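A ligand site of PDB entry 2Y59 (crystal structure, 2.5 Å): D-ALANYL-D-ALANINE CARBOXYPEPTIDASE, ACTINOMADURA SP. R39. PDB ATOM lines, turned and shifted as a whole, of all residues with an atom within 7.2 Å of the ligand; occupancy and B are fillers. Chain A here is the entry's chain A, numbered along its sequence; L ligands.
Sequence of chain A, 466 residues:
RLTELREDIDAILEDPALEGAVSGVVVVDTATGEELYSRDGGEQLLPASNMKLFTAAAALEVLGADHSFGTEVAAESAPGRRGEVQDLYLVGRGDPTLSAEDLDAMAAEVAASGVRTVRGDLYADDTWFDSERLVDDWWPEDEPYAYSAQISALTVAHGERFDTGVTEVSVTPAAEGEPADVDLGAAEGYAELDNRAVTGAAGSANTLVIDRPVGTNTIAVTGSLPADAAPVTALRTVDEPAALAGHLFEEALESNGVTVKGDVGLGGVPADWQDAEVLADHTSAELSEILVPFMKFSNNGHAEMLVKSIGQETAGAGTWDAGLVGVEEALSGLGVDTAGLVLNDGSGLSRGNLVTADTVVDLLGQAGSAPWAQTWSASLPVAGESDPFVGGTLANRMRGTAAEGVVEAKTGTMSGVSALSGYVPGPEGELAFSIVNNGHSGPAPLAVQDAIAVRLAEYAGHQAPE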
ATOM      1  N   PRO A  47      15.977  19.188  21.820  1.00  0.00           N
ATOM      2  CA  PRO A  47      17.008  18.301  21.335  1.00  0.00           C
ATOM      3  C   PRO A  47      17.116  16.911  22.005  1.00  0.00           C
ATOM      4  O   PRO A  47      17.933  16.079  21.542  1.00  0.00           O
ATOM      5  CB  PRO A  47      18.290  19.093  21.646  1.00  0.00           C
ATOM      6  CG  PRO A  47      17.917  20.019  22.722  1.00  0.00           C
ATOM      7  CD  PRO A  47      16.475  19.986  22.943  1.00  0.00           C
ATOM      8  N   ALA A  48      16.371  16.659  23.074  1.00  0.00           N
ATOM      9  CA  ALA A  48      16.611  15.469  23.899  1.00  0.00           C
ATOM     10  C   ALA A  48      18.129  15.289  24.164  1.00  0.00           C
ATOM     11  O   ALA A  48      18.814  16.271  24.464  1.00  0.00           O
ATOM     12  CB  ALA A  48      15.984  14.227  23.252  1.00  0.00           C
ATOM     13  N   SER A  49      18.673  14.072  24.050  1.00  0.00           N
ATOM     14  CA  SER A  49      20.113  13.853  24.322  1.00  0.00           C
ATOM     15  C   SER A  49      21.128  14.433  23.316  1.00  0.00           C
ATOM     16  O   SER A  49      22.319  14.326  23.565  1.00  0.00           O
ATOM     17  CB  SER A  49      20.441  12.383  24.589  1.00  0.00           C
ATOM     18  OG  SER A  49      19.666  11.908  25.676  1.00  0.00           O
ATOM     19  N   ASN A  50      20.680  15.029  22.212  1.00  0.00           N
ATOM     20  CA  ASN A  50      21.610  15.764  21.345  1.00  0.00           C
ATOM     21  C   ASN A  50      22.245  16.960  22.079  1.00  0.00           C
ATOM     22  O   ASN A  50      23.269  17.504  21.656  1.00  0.00           O
ATOM     23  CB  ASN A  50      20.992  16.242  20.027  1.00  0.00           C
ATOM     24  CG  ASN A  50      20.930  15.155  18.952  1.00  0.00           C
ATOM     25  OD1 ASN A  50      20.652  13.981  19.236  1.00  0.00           O
ATOM     26  ND2 ASN A  50      21.173  15.559  17.704  1.00  0.00           N
ATOM     27  N   MET A  51      21.637  17.373  23.194  1.00  0.00           N
ATOM     28  CA  MET A  51      22.166  18.439  24.034  1.00  0.00           C
ATOM     29  C   MET A  51      23.590  18.113  24.556  1.00  0.00           C
ATOM     30  O   MET A  51      24.416  19.012  24.803  1.00  0.00           O
ATOM     31  CB  MET A  51      21.156  18.756  25.161  1.00  0.00           C
ATOM     32  CG  MET A  51      21.486  19.988  25.978  1.00  0.00           C
ATOM     33  SD  MET A  51      21.844  21.457  25.004  1.00  0.00           S
ATOM     34  CE  MET A  51      20.215  22.068  24.661  1.00  0.00           C
ATOM     35  N   LYS A  52      23.861  16.812  24.706  1.00  0.00           N
ATOM     36  CA  LYS A  52      25.161  16.352  25.192  1.00  0.00           C
ATOM     37  C   LYS A  52      26.290  16.742  24.245  1.00  0.00           C
ATOM     38  O   LYS A  52      27.411  16.987  24.702  1.00  0.00           O
ATOM     39  CB  LYS A  52      25.160  14.849  25.449  1.00  0.00           C
ATOM     40  CG  LYS A  52      24.300  14.455  26.649  1.00  0.00           C
ATOM     41  CD  LYS A  52      24.142  12.971  26.719  1.00  0.00           C
ATOM     42  CE  LYS A  52      23.203  12.548  27.860  1.00  0.00           C
ATOM     43  NZ  LYS A  52      21.796  12.637  27.512  1.00  0.00           N
ATOM     44  N   ASP A 142       9.430  10.740  36.939  1.00  0.00           N
ATOM     45  CA  ASP A 142      10.638  10.161  36.337  1.00  0.00           C
ATOM     46  C   ASP A 142      11.772   9.898  37.331  1.00  0.00           C
ATOM     47  O   ASP A 142      12.777   9.294  36.978  1.00  0.00           O
ATOM     48  CB  ASP A 142      11.181  11.129  35.294  1.00  0.00           C
ATOM     49  CG  ASP A 142      10.462  11.057  33.968  1.00  0.00           C
ATOM     50  OD1 ASP A 142       9.651  10.127  33.748  1.00  0.00           O
ATOM     51  OD2 ASP A 142      10.741  11.932  33.128  1.00  0.00           O
ATOM     52  N   TYR A 145      14.040   6.471  37.930  1.00  0.00           N
ATOM     53  CA  TYR A 145      14.817   5.824  36.863  1.00  0.00           C
ATOM     54  C   TYR A 145      16.205   6.397  36.653  1.00  0.00           C
ATOM     55  O   TYR A 145      16.432   7.594  36.848  1.00  0.00           O
ATOM     56  CB  TYR A 145      13.992   5.751  35.564  1.00  0.00           C
ATOM     57  CG  TYR A 145      12.594   5.291  35.911  1.00  0.00           C
ATOM     58  CD1 TYR A 145      12.379   4.000  36.425  1.00  0.00           C
ATOM     59  CD2 TYR A 145      11.511   6.157  35.862  1.00  0.00           C
ATOM     60  CE1 TYR A 145      11.107   3.584  36.810  1.00  0.00           C
ATOM     61  CE2 TYR A 145      10.257   5.756  36.250  1.00  0.00           C
ATOM     62  CZ  TYR A 145      10.058   4.473  36.716  1.00  0.00           C
ATOM     63  OH  TYR A 145       8.808   4.088  37.102  1.00  0.00           O
ATOM     64  N   TYR A 147      18.261   7.465  34.461  1.00  0.00           N
ATOM     65  CA  TYR A 147      18.601   8.679  33.686  1.00  0.00           C
ATOM     66  C   TYR A 147      18.181   9.949  34.415  1.00  0.00           C
ATOM     67  O   TYR A 147      18.488  11.044  33.959  1.00  0.00           O
ATOM     68  CB  TYR A 147      17.907   8.645  32.330  1.00  0.00           C
ATOM     69  CG  TYR A 147      16.403   8.704  32.476  1.00  0.00           C
ATOM     70  CD1 TYR A 147      15.752   9.931  32.550  1.00  0.00           C
ATOM     71  CD2 TYR A 147      15.626   7.530  32.565  1.00  0.00           C
ATOM     72  CE1 TYR A 147      14.396  10.023  32.679  1.00  0.00           C
ATOM     73  CE2 TYR A 147      14.245   7.600  32.708  1.00  0.00           C
ATOM     74  CZ  TYR A 147      13.642   8.859  32.747  1.00  0.00           C
ATOM     75  OH  TYR A 147      12.292   9.006  32.893  1.00  0.00           O
ATOM     76  N   SER A 148      17.432   9.793  35.518  1.00  0.00           N
ATOM     77  CA  SER A 148      16.923  10.933  36.275  1.00  0.00           C
ATOM     78  C   SER A 148      17.492  11.014  37.675  1.00  0.00           C
ATOM     79  O   SER A 148      16.909  11.626  38.578  1.00  0.00           O
ATOM     80  CB  SER A 148      15.422  10.941  36.350  1.00  0.00           C
ATOM     81  OG  SER A 148      15.003  12.175  36.905  1.00  0.00           O
ATOM     82  N   PHE A 297      26.359   5.775  25.563  1.00  0.00           N
ATOM     83  CA  PHE A 297      25.112   5.338  26.199  1.00  0.00           C
ATOM     84  C   PHE A 297      24.241   6.502  26.675  1.00  0.00           C
ATOM     85  O   PHE A 297      23.157   6.287  27.252  1.00  0.00           O
ATOM     86  CB  PHE A 297      25.410   4.344  27.314  1.00  0.00           C
ATOM     87  CG  PHE A 297      26.281   3.186  26.889  1.00  0.00           C
ATOM     88  CD1 PHE A 297      25.806   2.210  26.009  1.00  0.00           C
ATOM     89  CD2 PHE A 297      27.570   3.056  27.370  1.00  0.00           C
ATOM     90  CE1 PHE A 297      26.608   1.133  25.619  1.00  0.00           C
ATOM     91  CE2 PHE A 297      28.373   1.991  26.987  1.00  0.00           C
ATOM     92  CZ  PHE A 297      27.888   1.019  26.117  1.00  0.00           C
ATOM     93  N   SER A 298      24.700   7.734  26.460  1.00  0.00           N
ATOM     94  CA  SER A 298      23.847   8.887  26.771  1.00  0.00           C
ATOM     95  C   SER A 298      23.611   8.913  28.298  1.00  0.00           C
ATOM     96  O   SER A 298      22.488   8.799  28.778  1.00  0.00           O
ATOM     97  CB  SER A 298      22.513   8.753  26.006  1.00  0.00           C
ATOM     98  OG  SER A 298      21.920  10.017  25.670  1.00  0.00           O
ATOM     99  N   ASN A 299      24.694   9.025  29.055  1.00  0.00           N
ATOM    100  CA  ASN A 299      24.592   9.093  30.516  1.00  0.00           C
ATOM    101  C   ASN A 299      24.217  10.501  30.950  1.00  0.00           C
ATOM    102  O   ASN A 299      24.993  11.412  30.705  1.00  0.00           O
ATOM    103  CB  ASN A 299      25.912   8.675  31.163  1.00  0.00           C
ATOM    104  CG  ASN A 299      25.757   8.386  32.625  1.00  0.00           C
ATOM    105  OD1 ASN A 299      26.064   7.288  33.071  1.00  0.00           O
ATOM    106  ND2 ASN A 299      25.299   9.346  33.385  1.00  0.00           N
ATOM    107  N   ASN A 300      23.041  10.648  31.564  1.00  0.00           N
ATOM    108  CA  ASN A 300      22.518  11.953  32.041  1.00  0.00           C
ATOM    109  C   ASN A 300      23.258  12.484  33.297  1.00  0.00           C
ATOM    110  O   ASN A 300      23.526  13.663  33.417  1.00  0.00           O
ATOM    111  CB  ASN A 300      21.002  11.890  32.312  1.00  0.00           C
ATOM    112  CG  ASN A 300      20.136  11.884  31.042  1.00  0.00           C
ATOM    113  OD1 ASN A 300      20.628  11.883  29.931  1.00  0.00           O
ATOM    114  ND2 ASN A 300      18.827  11.887  31.229  1.00  0.00           N
ATOM    115  N   SER A 347      22.318  17.460  29.969  1.00  0.00           N
ATOM    116  CA  SER A 347      21.939  16.137  29.467  1.00  0.00           C
ATOM    117  C   SER A 347      20.917  16.173  28.345  1.00  0.00           C
ATOM    118  O   SER A 347      20.925  15.319  27.476  1.00  0.00           O
ATOM    119  CB  SER A 347      21.378  15.256  30.606  1.00  0.00           C
ATOM    120  OG  SER A 347      20.101  15.693  31.013  1.00  0.00           O
ATOM    121  N   GLY A 348      20.047  17.150  28.369  1.00  0.00           N
ATOM    122  CA  GLY A 348      18.926  17.191  27.447  1.00  0.00           C
ATOM    123  C   GLY A 348      17.653  16.633  28.059  1.00  0.00           C
ATOM    124  O   GLY A 348      16.615  16.679  27.437  1.00  0.00           O
ATOM    125  N   LEU A 349      17.717  16.108  29.278  1.00  0.00           N
ATOM    126  CA  LEU A 349      16.516  15.597  29.883  1.00  0.00           C
ATOM    127  C   LEU A 349      15.462  16.710  29.912  1.00  0.00           C
ATOM    128  O   LEU A 349      14.273  16.433  29.781  1.00  0.00           O
ATOM    129  CB  LEU A 349      16.785  15.127  31.311  1.00  0.00           C
ATOM    130  CG  LEU A 349      16.014  13.927  31.831  1.00  0.00           C
ATOM    131  CD1 LEU A 349      15.641  14.111  33.298  1.00  0.00           C
ATOM    132  CD2 LEU A 349      14.752  13.588  31.005  1.00  0.00           C
ATOM    133  N   SER A 350      15.901  17.946  30.132  1.00  0.00           N
ATOM    134  CA  SER A 350      14.986  19.067  30.329  1.00  0.00           C
ATOM    135  C   SER A 350      14.245  19.489  29.053  1.00  0.00           C
ATOM    136  O   SER A 350      14.846  19.597  27.983  1.00  0.00           O
ATOM    137  CB  SER A 350      15.708  20.279  30.917  1.00  0.00           C
ATOM    138  OG  SER A 350      14.852  21.425  30.938  1.00  0.00           O
ATOM    139  N   THR A 393      23.990   3.567  21.605  1.00  0.00           N
ATOM    140  CA  THR A 393      22.580   3.603  21.253  1.00  0.00           C
ATOM    141  C   THR A 393      22.300   3.385  19.749  1.00  0.00           C
ATOM    142  O   THR A 393      21.141   3.364  19.329  1.00  0.00           O
ATOM    143  CB  THR A 393      21.950   4.914  21.712  1.00  0.00           C
ATOM    144  OG1 THR A 393      22.574   5.983  21.017  1.00  0.00           O
ATOM    145  CG2 THR A 393      22.101   5.089  23.236  1.00  0.00           C
ATOM    146  N   LYS A 410      24.899  11.102  17.409  1.00  0.00           N
ATOM    147  CA  LYS A 410      24.315  11.018  18.736  1.00  0.00           C
ATOM    148  C   LYS A 410      22.817  10.989  18.578  1.00  0.00           C
ATOM    149  O   LYS A 410      22.289  11.677  17.703  1.00  0.00           O
ATOM    150  CB  LYS A 410      24.753  12.192  19.653  1.00  0.00           C
ATOM    151  CG  LYS A 410      24.109  12.216  21.058  1.00  0.00           C
ATOM    152  CD  LYS A 410      24.744  11.202  21.993  1.00  0.00           C
ATOM    153  CE  LYS A 410      23.983  11.037  23.326  1.00  0.00           C
ATOM    154  NZ  LYS A 410      22.672  10.388  23.111  1.00  0.00           N
ATOM    155  N   THR A 411      22.159  10.216  19.444  1.00  0.00           N
ATOM    156  CA  THR A 411      20.741  10.021  19.426  1.00  0.00           C
ATOM    157  C   THR A 411      20.041  10.880  20.464  1.00  0.00           C
ATOM    158  O   THR A 411      20.686  11.521  21.294  1.00  0.00           O
ATOM    159  CB  THR A 411      20.365   8.554  19.653  1.00  0.00           C
ATOM    160  OG1 THR A 411      20.995   8.066  20.851  1.00  0.00           O
ATOM    161  CG2 THR A 411      20.788   7.712  18.473  1.00  0.00           C
ATOM    162  N   GLY A 412      18.715  10.880  20.428  1.00  0.00           N
ATOM    163  CA  GLY A 412      17.981  11.765  21.298  1.00  0.00           C
ATOM    164  C   GLY A 412      16.549  11.346  21.221  1.00  0.00           C
ATOM    165  O   GLY A 412      15.990  11.363  20.150  1.00  0.00           O
ATOM    166  N   THR A 413      15.973  10.926  22.335  1.00  0.00           N
ATOM    167  CA  THR A 413      14.584  10.504  22.335  1.00  0.00           C
ATOM    168  C   THR A 413      13.867  10.765  23.674  1.00  0.00           C
ATOM    169  O   THR A 413      14.434  10.495  24.739  1.00  0.00           O
ATOM    170  CB  THR A 413      14.414   8.987  21.905  1.00  0.00           C
ATOM    171  OG1 THR A 413      15.131   8.708  20.677  1.00  0.00           O
ATOM    172  CG2 THR A 413      12.936   8.634  21.676  1.00  0.00           C
ATOM    173  N   MET A 414      12.660  11.341  23.582  1.00  0.00           N
ATOM    174  CA  MET A 414      11.621  11.281  24.638  1.00  0.00           C
ATOM    175  C   MET A 414      10.250  11.481  23.955  1.00  0.00           C
ATOM    176  O   MET A 414      10.225  11.595  22.737  1.00  0.00           O
ATOM    177  CB  MET A 414      11.880  12.297  25.783  1.00  0.00           C
ATOM    178  CG  MET A 414      11.922  13.772  25.422  1.00  0.00           C
ATOM    179  SD  MET A 414      12.405  14.737  26.884  1.00  0.00           S
ATOM    180  CE  MET A 414      13.749  15.723  26.243  1.00  0.00           C
ATOM    181  N   SER A 415       9.127  11.521  24.691  1.00  0.00           N
ATOM    182  CA  SER A 415       7.833  11.806  24.036  1.00  0.00           C
ATOM    183  C   SER A 415       7.966  12.931  23.010  1.00  0.00           C
ATOM    184  O   SER A 415       8.429  14.012  23.341  1.00  0.00           O
ATOM    185  CB  SER A 415       6.765  12.258  25.003  1.00  0.00           C
ATOM    186  OG  SER A 415       5.959  11.191  25.409  1.00  0.00           O
ATOM    187  N   VAL A 417       9.889  13.800  20.723  1.00  0.00           N
ATOM    188  CA  VAL A 417      11.209  14.315  20.372  1.00  0.00           C
ATOM    189  C   VAL A 417      12.145  13.165  20.061  1.00  0.00           C
ATOM    190  O   VAL A 417      12.262  12.209  20.833  1.00  0.00           O
ATOM    191  CB  VAL A 417      11.835  15.194  21.481  1.00  0.00           C
ATOM    192  CG1 VAL A 417      13.283  15.573  21.162  1.00  0.00           C
ATOM    193  CG2 VAL A 417      11.019  16.434  21.684  1.00  0.00           C
ATOM    194  N   SER A 418      12.826  13.282  18.933  1.00  0.00           N
ATOM    195  CA  SER A 418      13.821  12.332  18.497  1.00  0.00           C
ATOM    196  C   SER A 418      14.815  13.148  17.696  1.00  0.00           C
ATOM    197  O   SER A 418      14.432  14.159  17.092  1.00  0.00           O
ATOM    198  CB  SER A 418      13.177  11.255  17.627  1.00  0.00           C
ATOM    199  OG  SER A 418      14.070  10.168  17.354  1.00  0.00           O
ATOM    200  N   ALA A 419      16.076  12.731  17.723  1.00  0.00           N
ATOM    201  CA  ALA A 419      17.128  13.466  17.073  1.00  0.00           C
ATOM    202  C   ALA A 419      18.257  12.517  16.740  1.00  0.00           C
ATOM    203  O   ALA A 419      18.470  11.494  17.447  1.00  0.00           O
ATOM    204  CB  ALA A 419      17.610  14.574  17.974  1.00  0.00           C
HETATM  205  O1  LIG L   1      17.002  11.254  28.982  1.00  0.00           O
HETATM  206  C1  LIG L   1      16.455  10.596  28.113  1.00  0.00           C
HETATM  207  N1  LIG L   1      16.429  10.951  26.848  1.00  0.00           N
HETATM  208  C2  LIG L   1      17.052  12.126  26.302  1.00  0.00           C
HETATM  209  B1  LIG L   1      18.259  11.400  25.553  1.00  0.00           B
HETATM  210  O2  LIG L   1      17.925  11.305  24.064  1.00  0.00           O
HETATM  211  O3  LIG L   1      18.641  10.025  26.152  1.00  0.00           O
HETATM  212  C3  LIG L   1      15.866   9.315  28.525  1.00  0.00           C
HETATM  213  C4  LIG L   1      14.597   9.137  29.067  1.00  0.00           C
HETATM  214  N2  LIG L   1      13.704  10.164  29.226  1.00  0.00           N
HETATM  215  O4  LIG L   1      12.438   9.913  29.756  1.00  0.00           O
HETATM  216  O5  LIG L   1      14.041  11.465  28.864  1.00  0.00           O
HETATM  217  C5  LIG L   1      16.738   8.254  28.387  1.00  0.00           C
HETATM  218  C6  LIG L   1      16.352   6.977  28.754  1.00  0.00           C
HETATM  219  C7  LIG L   1      15.088   6.779  29.288  1.00  0.00           C
HETATM  220  C8  LIG L   1      14.211   7.861  29.434  1.00  0.00           C
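OG of Ser 298 sits at hydrogen-bond distance from O3 of the ligand (3.3 Å).
The backbone carbonyl oxygen (O) of Thr 413 sits at hydrogen-bond distance from a nitrogen (N1) of the ligand, at 2.9 Å.
OG of Ser 49 is bonded to B1 of the ligand, 1.5 Å away.
OH of Tyr 147 lies within hydrogen-bond range of O4 of the ligand.
The side-chain amide nitrogen of Asn 300 is in hydrogen-bond range of an oxygen (O1) of the ligand (3.0 Å).
O2 of the ligand is in hydrogen-bond range of N of Thr 413, at 2.6 Å.
N of Ser 49 sits close to O2 of the ligand (2.9 Å).
Residues that only touch the ligand: Ala 48 (3.6 Å), Leu 349 (3.1 Å), Thr 411 (3.9 Å), Gly 412 (2.8 Å) and Met 414 (3.9 Å).
Hydrophobic or aromatic side chains within 4 Å of the ligand: Ala 48, Tyr 147, Leu 349 and Met 414.
The side-chain hydroxyl (OG) of Ser 347 lies within hydrogen-bond range of the backbone NH (N) of Leu 349, 3.0 Å away.
O of Gly 412 lies within hydrogen-bond range of N of Ala 419 (2.8 Å).
The side-chain hydroxyl (OH) of Tyr 147 sits close to the side-chain carboxylate (OD1) of Asp 142, at 3.0 Å.
The side-chain amide oxygen (OD1) of Asn 300 is in hydrogen-bond range of the side-chain amino group (NZ) of Lys 52 (2.8 Å).
The backbone carbonyl oxygen of Thr 411 lies close to the side-chain amide oxygen of Asn 50 (3.2 Å).
NZ of Lys 52 lies within hydrogen-bond range of OG of Ser 49 (2.9 Å).
The side-chain hydroxyl (OG1) of Thr 393 sits at hydrogen-bond distance from the side-chain hydroxyl (OG1) of Thr 411, 2.6 Å away.
ND2 of Asn 300 is in hydrogen-bond range of O of Tyr 147.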
